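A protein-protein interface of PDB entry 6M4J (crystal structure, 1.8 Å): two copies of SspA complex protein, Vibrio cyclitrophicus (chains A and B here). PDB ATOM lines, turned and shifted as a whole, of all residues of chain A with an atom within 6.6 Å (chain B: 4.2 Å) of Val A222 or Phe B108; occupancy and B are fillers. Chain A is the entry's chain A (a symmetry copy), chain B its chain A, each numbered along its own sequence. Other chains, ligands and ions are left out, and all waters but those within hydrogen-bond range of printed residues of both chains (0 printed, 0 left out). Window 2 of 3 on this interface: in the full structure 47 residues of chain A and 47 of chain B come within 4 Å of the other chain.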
ATOM      1  N   LEU A  76      21.297 -11.545  25.157  1.00  0.00           N
ATOM      2  CA  LEU A  76      22.286 -10.752  24.406  1.00  0.00           C
ATOM      3  C   LEU A  76      23.235 -11.648  23.612  1.00  0.00           C
ATOM      4  O   LEU A  76      23.452 -11.418  22.425  1.00  0.00           O
ATOM      5  CB  LEU A  76      23.069  -9.829  25.336  1.00  0.00           C
ATOM      6  CG  LEU A  76      24.201  -9.019  24.664  1.00  0.00           C
ATOM      7  CD1 LEU A  76      23.698  -8.162  23.507  1.00  0.00           C
ATOM      8  CD2 LEU A  76      24.889  -8.151  25.703  1.00  0.00           C
ATOM      9  N   LYS A  79      20.692 -13.555  20.736  1.00  0.00           N
ATOM     10  CA  LYS A  79      20.064 -12.616  19.802  1.00  0.00           C
ATOM     11  C   LYS A  79      21.083 -11.662  19.192  1.00  0.00           C
ATOM     12  O   LYS A  79      20.920 -11.216  18.055  1.00  0.00           O
ATOM     13  CB  LYS A  79      18.946 -11.828  20.485  1.00  0.00           C
ATOM     14  CG  LYS A  79      17.762 -12.688  20.893  1.00  0.00           C
ATOM     15  CD  LYS A  79      16.840 -11.928  21.831  1.00  0.00           C
ATOM     16  CE  LYS A  79      15.605 -12.742  22.143  1.00  0.00           C
ATOM     17  NZ  LYS A  79      14.597 -11.913  22.850  1.00  0.00           N
ATOM     18  N   GLY A  80      22.139 -11.366  19.944  1.00  0.00           N
ATOM     19  CA  GLY A  80      23.199 -10.480  19.458  1.00  0.00           C
ATOM     20  C   GLY A  80      23.847 -11.031  18.200  1.00  0.00           C
ATOM     21  O   GLY A  80      24.260 -10.261  17.328  1.00  0.00           O
ATOM     22  N   LEU A  81      23.953 -12.361  18.106  1.00  0.00           N
ATOM     23  CA  LEU A  81      24.522 -12.998  16.912  1.00  0.00           C
ATOM     24  C   LEU A  81      23.439 -13.224  15.873  1.00  0.00           C
ATOM     25  O   LEU A  81      23.645 -13.021  14.675  1.00  0.00           O
ATOM     26  CB  LEU A  81      25.212 -14.320  17.244  1.00  0.00           C
ATOM     27  CG  LEU A  81      26.544 -14.209  17.993  1.00  0.00           C
ATOM     28  CD1 LEU A  81      27.146 -15.588  18.233  1.00  0.00           C
ATOM     29  CD2 LEU A  81      27.527 -13.315  17.247  1.00  0.00           C
ATOM     30  N   ALA A  82      22.285 -13.674  16.343  1.00  0.00           N
ATOM     31  CA  ALA A  82      21.208 -14.020  15.446  1.00  0.00           C
ATOM     32  C   ALA A  82      20.737 -12.802  14.707  1.00  0.00           C
ATOM     33  O   ALA A  82      20.355 -12.907  13.577  1.00  0.00           O
ATOM     34  CB  ALA A  82      20.040 -14.642  16.182  1.00  0.00           C
ATOM     35  N   PHE A  83      20.670 -11.665  15.374  1.00  0.00           N
ATOM     36  CA  PHE A  83      20.039 -10.538  14.718  1.00  0.00           C
ATOM     37  C   PHE A  83      20.948  -9.934  13.650  1.00  0.00           C
ATOM     38  O   PHE A  83      20.561  -8.999  12.975  1.00  0.00           O
ATOM     39  CB  PHE A  83      19.528  -9.469  15.708  1.00  0.00           C
ATOM     40  CG  PHE A  83      18.367  -9.900  16.592  1.00  0.00           C
ATOM     41  CD1 PHE A  83      17.951  -9.093  17.649  1.00  0.00           C
ATOM     42  CD2 PHE A  83      17.711 -11.101  16.389  1.00  0.00           C
ATOM     43  CE1 PHE A  83      16.899  -9.473  18.463  1.00  0.00           C
ATOM     44  CE2 PHE A  83      16.659 -11.482  17.191  1.00  0.00           C
ATOM     45  CZ  PHE A  83      16.250 -10.674  18.236  1.00  0.00           C
ATOM     46  N   LYS A  84      22.169 -10.437  13.523  1.00  0.00           N
ATOM     47  CA  LYS A  84      22.915 -10.070  12.340  1.00  0.00           C
ATOM     48  C   LYS A  84      22.674 -10.981  11.130  1.00  0.00           C
ATOM     49  O   LYS A  84      23.255 -10.750  10.062  1.00  0.00           O
ATOM     50  CB  LYS A  84      24.392 -10.017  12.652  1.00  0.00           C
ATOM     51  CG  LYS A  84      25.110  -8.928  11.902  1.00  0.00           C
ATOM     52  CD  LYS A  84      25.317  -7.700  12.772  1.00  0.00           C
ATOM     53  CE  LYS A  84      25.868  -6.543  11.956  1.00  0.00           C
ATOM     54  NZ  LYS A  84      24.959  -6.183  10.834  1.00  0.00           N
ATOM     55  N   LEU A  86      19.334 -11.979   9.988  1.00  0.00           N
ATOM     56  CA  LEU A  86      17.898 -12.101   9.831  1.00  0.00           C
ATOM     57  C   LEU A  86      17.491 -12.612   8.450  1.00  0.00           C
ATOM     58  O   LEU A  86      16.424 -13.154   8.271  1.00  0.00           O
ATOM     59  CB  LEU A  86      17.248 -10.772  10.145  1.00  0.00           C
ATOM     60  CG  LEU A  86      17.424 -10.343  11.604  1.00  0.00           C
ATOM     61  CD1 LEU A  86      16.810  -8.968  11.793  1.00  0.00           C
ATOM     62  CD2 LEU A  86      16.756 -11.344  12.526  1.00  0.00           C
ATOM     63  N   SER A 219      33.459  -6.105  18.953  1.00  0.00           N
ATOM     64  CA  SER A 219      32.338  -7.016  18.757  1.00  0.00           C
ATOM     65  C   SER A 219      31.270  -6.447  17.829  1.00  0.00           C
ATOM     66  O   SER A 219      30.878  -5.282  17.930  1.00  0.00           O
ATOM     67  CB  SER A 219      31.713  -7.393  20.102  1.00  0.00           C
ATOM     68  OG  SER A 219      30.392  -7.864  19.903  1.00  0.00           O
ATOM     69  N   GLU A 220      30.782  -7.288  16.932  1.00  0.00           N
ATOM     70  CA  GLU A 220      29.690  -6.897  16.068  1.00  0.00           C
ATOM     71  C   GLU A 220      28.340  -7.365  16.593  1.00  0.00           C
ATOM     72  O   GLU A 220      27.364  -7.337  15.861  1.00  0.00           O
ATOM     73  CB  GLU A 220      29.900  -7.473  14.689  1.00  0.00           C
ATOM     74  CG  GLU A 220      31.153  -6.979  13.991  1.00  0.00           C
ATOM     75  CD  GLU A 220      31.146  -7.385  12.523  1.00  0.00           C
ATOM     76  OE1 GLU A 220      30.532  -6.682  11.696  1.00  0.00           O
ATOM     77  OE2 GLU A 220      31.732  -8.439  12.201  1.00  0.00           O
ATOM     78  N   LEU A 221      28.281  -7.758  17.866  1.00  0.00           N
ATOM     79  CA  LEU A 221      27.023  -8.195  18.464  1.00  0.00           C
ATOM     80  C   LEU A 221      26.015  -7.090  18.332  1.00  0.00           C
ATOM     81  O   LEU A 221      26.352  -5.936  18.545  1.00  0.00           O
ATOM     82  CB  LEU A 221      27.191  -8.431  19.951  1.00  0.00           C
ATOM     83  CG  LEU A 221      27.683  -9.747  20.547  1.00  0.00           C
ATOM     84  CD1 LEU A 221      27.682  -9.575  22.059  1.00  0.00           C
ATOM     85  CD2 LEU A 221      26.866 -10.979  20.150  1.00  0.00           C
ATOM     86  N   VAL A 222      24.781  -7.434  17.990  1.00  0.00           N
ATOM     87  CA  VAL A 222      23.689  -6.469  17.966  1.00  0.00           C
ATOM     88  C   VAL A 222      23.215  -6.246  19.414  1.00  0.00           C
ATOM     89  O   VAL A 222      22.808  -7.202  20.082  1.00  0.00           O
ATOM     90  CB  VAL A 222      22.515  -6.955  17.073  1.00  0.00           C
ATOM     91  CG1 VAL A 222      21.345  -5.989  17.180  1.00  0.00           C
ATOM     92  CG2 VAL A 222      22.954  -7.081  15.627  1.00  0.00           C
ATOM     93  N   PRO A 223      23.292  -4.996  19.910  1.00  0.00           N
ATOM     94  CA  PRO A 223      22.835  -4.677  21.260  1.00  0.00           C
ATOM     95  C   PRO A 223      21.372  -5.089  21.464  1.00  0.00           C
ATOM     96  O   PRO A 223      20.543  -4.909  20.562  1.00  0.00           O
ATOM     97  CB  PRO A 223      22.992  -3.155  21.325  1.00  0.00           C
ATOM     98  CG  PRO A 223      24.112  -2.872  20.372  1.00  0.00           C
ATOM     99  CD  PRO A 223      23.867  -3.818  19.231  1.00  0.00           C
ATOM    100  N   LEU A 224      21.087  -5.693  22.616  1.00  0.00           N
ATOM    101  CA  LEU A 224      19.720  -6.031  23.016  1.00  0.00           C
ATOM    102  C   LEU A 224      19.026  -4.747  23.480  1.00  0.00           C
ATOM    103  O   LEU A 224      17.896  -4.449  23.075  1.00  0.00           O
ATOM    104  CB  LEU A 224      19.744  -7.086  24.139  1.00  0.00           C
ATOM    105  CG  LEU A 224      18.500  -7.927  24.448  1.00  0.00           C
ATOM    106  CD1 LEU A 224      18.264  -8.971  23.366  1.00  0.00           C
ATOM    107  CD2 LEU A 224      18.635  -8.566  25.821  1.00  0.00           C
ATOM    108  N   ILE A 225      19.714  -3.989  24.329  1.00  0.00           N
ATOM    109  CA  ILE A 225      19.232  -2.677  24.745  1.00  0.00           C
ATOM    110  C   ILE A 225      20.120  -1.609  24.101  1.00  0.00           C
ATOM    111  O   ILE A 225      21.275  -1.453  24.486  1.00  0.00           O
ATOM    112  CB  ILE A 225      19.234  -2.550  26.284  1.00  0.00           C
ATOM    113  CG1 ILE A 225      18.378  -3.671  26.896  1.00  0.00           C
ATOM    114  CG2 ILE A 225      18.725  -1.179  26.736  1.00  0.00           C
ATOM    115  CD1 ILE A 225      18.590  -3.843  28.384  1.00  0.00           C
ATOM    116  N   HIS A 226      19.594  -0.912  23.101  1.00  0.00           N
ATOM    117  CA  HIS A 226      20.305   0.245  22.550  1.00  0.00           C
ATOM    118  C   HIS A 226      20.174   1.390  23.506  1.00  0.00           C
ATOM    119  O   HIS A 226      19.118   1.596  24.093  1.00  0.00           O
ATOM    120  CB  HIS A 226      19.767   0.614  21.176  1.00  0.00           C
ATOM    121  CG  HIS A 226      20.198  -0.328  20.095  1.00  0.00           C
ATOM    122  ND1 HIS A 226      21.274  -0.098  19.315  1.00  0.00           N
ATOM    123  CD2 HIS A 226      19.674  -1.543  19.698  1.00  0.00           C
ATOM    124  CE1 HIS A 226      21.419  -1.126  18.456  1.00  0.00           C
ATOM    125  NE2 HIS A 226      20.439  -2.008  18.698  1.00  0.00           N
ATOM    126  N   LEU A 234      27.299  -1.712  23.760  1.00  0.00           N
ATOM    127  CA  LEU A 234      26.660  -3.049  23.695  1.00  0.00           C
ATOM    128  C   LEU A 234      25.421  -3.234  24.576  1.00  0.00           C
ATOM    129  O   LEU A 234      24.604  -4.126  24.313  1.00  0.00           O
ATOM    130  CB  LEU A 234      27.665  -4.165  23.998  1.00  0.00           C
ATOM    131  CG  LEU A 234      28.855  -4.255  23.042  1.00  0.00           C
ATOM    132  CD1 LEU A 234      29.936  -5.134  23.648  1.00  0.00           C
ATOM    133  CD2 LEU A 234      28.424  -4.771  21.670  1.00  0.00           C
ATOM    134  N   PHE B  83       9.806  -6.375  15.759  1.00  0.00           N
ATOM    135  CA  PHE B  83      10.303  -7.711  15.496  1.00  0.00           C
ATOM    136  C   PHE B  83       9.176  -8.652  15.077  1.00  0.00           C
ATOM    137  O   PHE B  83       9.422  -9.807  14.783  1.00  0.00           O
ATOM    138  CB  PHE B  83      11.128  -8.290  16.666  1.00  0.00           C
ATOM    139  CG  PHE B  83      12.457  -7.598  16.932  1.00  0.00           C
ATOM    140  CD1 PHE B  83      13.194  -7.906  18.074  1.00  0.00           C
ATOM    141  CD2 PHE B  83      12.957  -6.639  16.070  1.00  0.00           C
ATOM    142  CE1 PHE B  83      14.402  -7.284  18.330  1.00  0.00           C
ATOM    143  CE2 PHE B  83      14.162  -6.020  16.316  1.00  0.00           C
ATOM    144  CZ  PHE B  83      14.889  -6.333  17.450  1.00  0.00           C
ATOM    145  N   ASN B 104      18.896   5.587  18.905  1.00  0.00           N
ATOM    146  CA  ASN B 104      19.767   4.480  18.547  1.00  0.00           C
ATOM    147  C   ASN B 104      19.015   3.187  18.255  1.00  0.00           C
ATOM    148  O   ASN B 104      19.397   2.465  17.328  1.00  0.00           O
ATOM    149  CB  ASN B 104      20.881   4.303  19.575  1.00  0.00           C
ATOM    150  CG  ASN B 104      21.893   5.435  19.512  1.00  0.00           C
ATOM    151  OD1 ASN B 104      22.066   6.072  18.465  1.00  0.00           O
ATOM    152  ND2 ASN B 104      22.545   5.711  20.635  1.00  0.00           N
ATOM    153  N   THR B 105      17.935   2.914  18.974  1.00  0.00           N
ATOM    154  CA  THR B 105      17.123   1.765  18.559  1.00  0.00           C
ATOM    155  C   THR B 105      16.450   1.949  17.199  1.00  0.00           C
ATOM    156  O   THR B 105      16.397   1.014  16.397  1.00  0.00           O
ATOM    157  CB  THR B 105      16.185   1.167  19.651  1.00  0.00           C
ATOM    158  OG1 THR B 105      14.810   1.122  19.225  1.00  0.00           O
ATOM    159  CG2 THR B 105      16.361   1.787  20.978  1.00  0.00           C
ATOM    160  N   CYS B 106      15.983   3.161  16.909  1.00  0.00           N
ATOM    161  CA  CYS B 106      15.413   3.451  15.598  1.00  0.00           C
ATOM    162  C   CYS B 106      16.473   3.388  14.488  1.00  0.00           C
ATOM    163  O   CYS B 106      16.188   2.950  13.367  1.00  0.00           O
ATOM    164  CB  CYS B 106      14.730   4.820  15.613  1.00  0.00           C
ATOM    165  SG  CYS B 106      13.195   4.865  16.567  1.00  0.00           S
ATOM    166  N   GLY B 107      17.692   3.825  14.803  1.00  0.00           N
ATOM    167  CA  GLY B 107      18.809   3.732  13.870  1.00  0.00           C
ATOM    168  C   GLY B 107      19.094   2.290  13.501  1.00  0.00           C
ATOM    169  O   GLY B 107      19.341   1.969  12.344  1.00  0.00           O
ATOM    170  N   PHE B 108      19.043   1.415  14.497  1.00  0.00           N
ATOM    171  CA  PHE B 108      19.205  -0.006  14.267  1.00  0.00           C
ATOM    172  C   PHE B 108      18.102  -0.570  13.361  1.00  0.00           C
ATOM    173  O   PHE B 108      18.363  -1.341  12.434  1.00  0.00           O
ATOM    174  CB  PHE B 108      19.230  -0.769  15.590  1.00  0.00           C
ATOM    175  CG  PHE B 108      19.106  -2.248  15.399  1.00  0.00           C
ATOM    176  CD1 PHE B 108      20.138  -2.951  14.798  1.00  0.00           C
ATOM    177  CD2 PHE B 108      17.938  -2.915  15.728  1.00  0.00           C
ATOM    178  CE1 PHE B 108      20.033  -4.310  14.568  1.00  0.00           C
ATOM    179  CE2 PHE B 108      17.826  -4.276  15.503  1.00  0.00           C
ATOM    180  CZ  PHE B 108      18.874  -4.973  14.919  1.00  0.00           C
ATOM    181  N   LEU B 109      16.862  -0.216  13.666  1.00  0.00           N
ATOM    182  CA  LEU B 109      15.761  -0.617  12.815  1.00  0.00           C
ATOM    183  C   LEU B 109      15.982  -0.188  11.363  1.00  0.00           C
ATOM    184  O   LEU B 109      15.744  -0.970  10.454  1.00  0.00           O
ATOM    185  CB  LEU B 109      14.429  -0.088  13.349  1.00  0.00           C
ATOM    186  CG  LEU B 109      13.965  -0.645  14.702  1.00  0.00           C
ATOM    187  CD1 LEU B 109      12.561  -0.137  15.005  1.00  0.00           C
ATOM    188  CD2 LEU B 109      14.014  -2.173  14.739  1.00  0.00           C
ATOM    189  N   GLU B 110      16.474   1.031  11.141  1.00  0.00           N
ATOM    190  CA  GLU B 110      16.797   1.466   9.775  1.00  0.00           C
ATOM    191  C   GLU B 110      17.816   0.543   9.125  1.00  0.00           C
ATOM    192  O   GLU B 110      17.708   0.235   7.937  1.00  0.00           O
ATOM    193  CB  GLU B 110      17.306   2.907   9.736  1.00  0.00           C
ATOM    194  CG  GLU B 110      16.222   3.944   9.957  1.00  0.00           C
ATOM    195  CD  GLU B 110      16.770   5.349   9.968  1.00  0.00           C
ATOM    196  OE1 GLU B 110      16.621   6.040   8.951  1.00  0.00           O
ATOM    197  OE2 GLU B 110      17.359   5.759  10.991  1.00  0.00           O
ATOM    198  N   SER B 111      18.774   0.082   9.923  1.00  0.00           N
ATOM    199  CA  SER B 111      19.872  -0.746   9.433  1.00  0.00           C
ATOM    200  C   SER B 111      19.412  -2.138   9.008  1.00  0.00           C
ATOM    201  O   SER B 111      20.126  -2.825   8.276  1.00  0.00           O
ATOM    202  CB  SER B 111      20.987  -0.844  10.479  1.00  0.00           C
ATOM    203  OG  SER B 111      20.738  -1.895  11.400  1.00  0.00           O
ATOM    204  N   ILE B 112      18.232  -2.550   9.474  1.00  0.00           N
ATOM    205  CA  ILE B 112      17.656  -3.824   9.055  1.00  0.00           C
ATOM    206  C   ILE B 112      16.430  -3.613   8.163  1.00  0.00           C
ATOM    207  O   ILE B 112      15.626  -4.519   7.978  1.00  0.00           O
ATOM    208  CB  ILE B 112      17.345  -4.786  10.233  1.00  0.00           C
ATOM    209  CG1 ILE B 112      16.406  -4.142  11.252  1.00  0.00           C
ATOM    210  CG2 ILE B 112      18.623  -5.286  10.905  1.00  0.00           C
ATOM    211  CD1 ILE B 112      15.813  -5.137  12.222  1.00  0.00           C
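O of Phe B108 sits at hydrogen-bond distance from OG of Ser B111, 2.6 Å away.
The backbone carbonyl oxygen of Gly A80 lies within hydrogen-bond range of the backbone NH of Val A222, 2.9 Å away.
NE2 of His A226 sits at hydrogen-bond distance from O of Pro A223, at 3.4 Å.
Phe A83 touches its own counterpart, Phe B83.
Of the 6 pairs that touch across the chains among the printed residues, 1 has its exchanged pair printed and touching as well.
Of the printed residues of chain B, Leu A86 touches Ile B112.
Printed residues of chain B within 4 Å of His A226: Asn B104, Thr B105 and Phe B108.
Printed residues of chain A within 4 Å of Asn B104: His A226 (3.7 Å).
Glu B110 touches none of the printed residues of chain A.
Gly B107 touches none of the printed residues of chain A.
The nearest printed residue of chain B that does not touch Val A222 is Phe B83 (6.5 Å).
Phe B83 touches Phe A83 (CE1 to CE1, 3.3 Å).
Ile B112 touches Leu A86.
Phe B108 touches Val A222.
Asn B104 touches His A226.
Thr B105 touches His A226.
Phe B108 touches His A226.
Of the 17 printed residues of chain A, 4 touch a printed residue of chain B.
Hydrophobic or aromatic side chains of chain A within 4 Å of the printed part of chain B: Phe A83, Leu A86, Val A222 and His A226.
Of the 10 printed residues of chain B, 5 touch a printed residue of chain A.
Hydrophobic or aromatic side chains of chain B within 4 Å of the printed part of chain A: Phe B83, Phe B108 and Ile B112.
Among the printed residues, 6 pairs touch across the chains.
Among the printed residues, no Asp or Glu carboxylate lies within 4 Å of a Lys or Arg side-chain nitrogen of the other chain.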
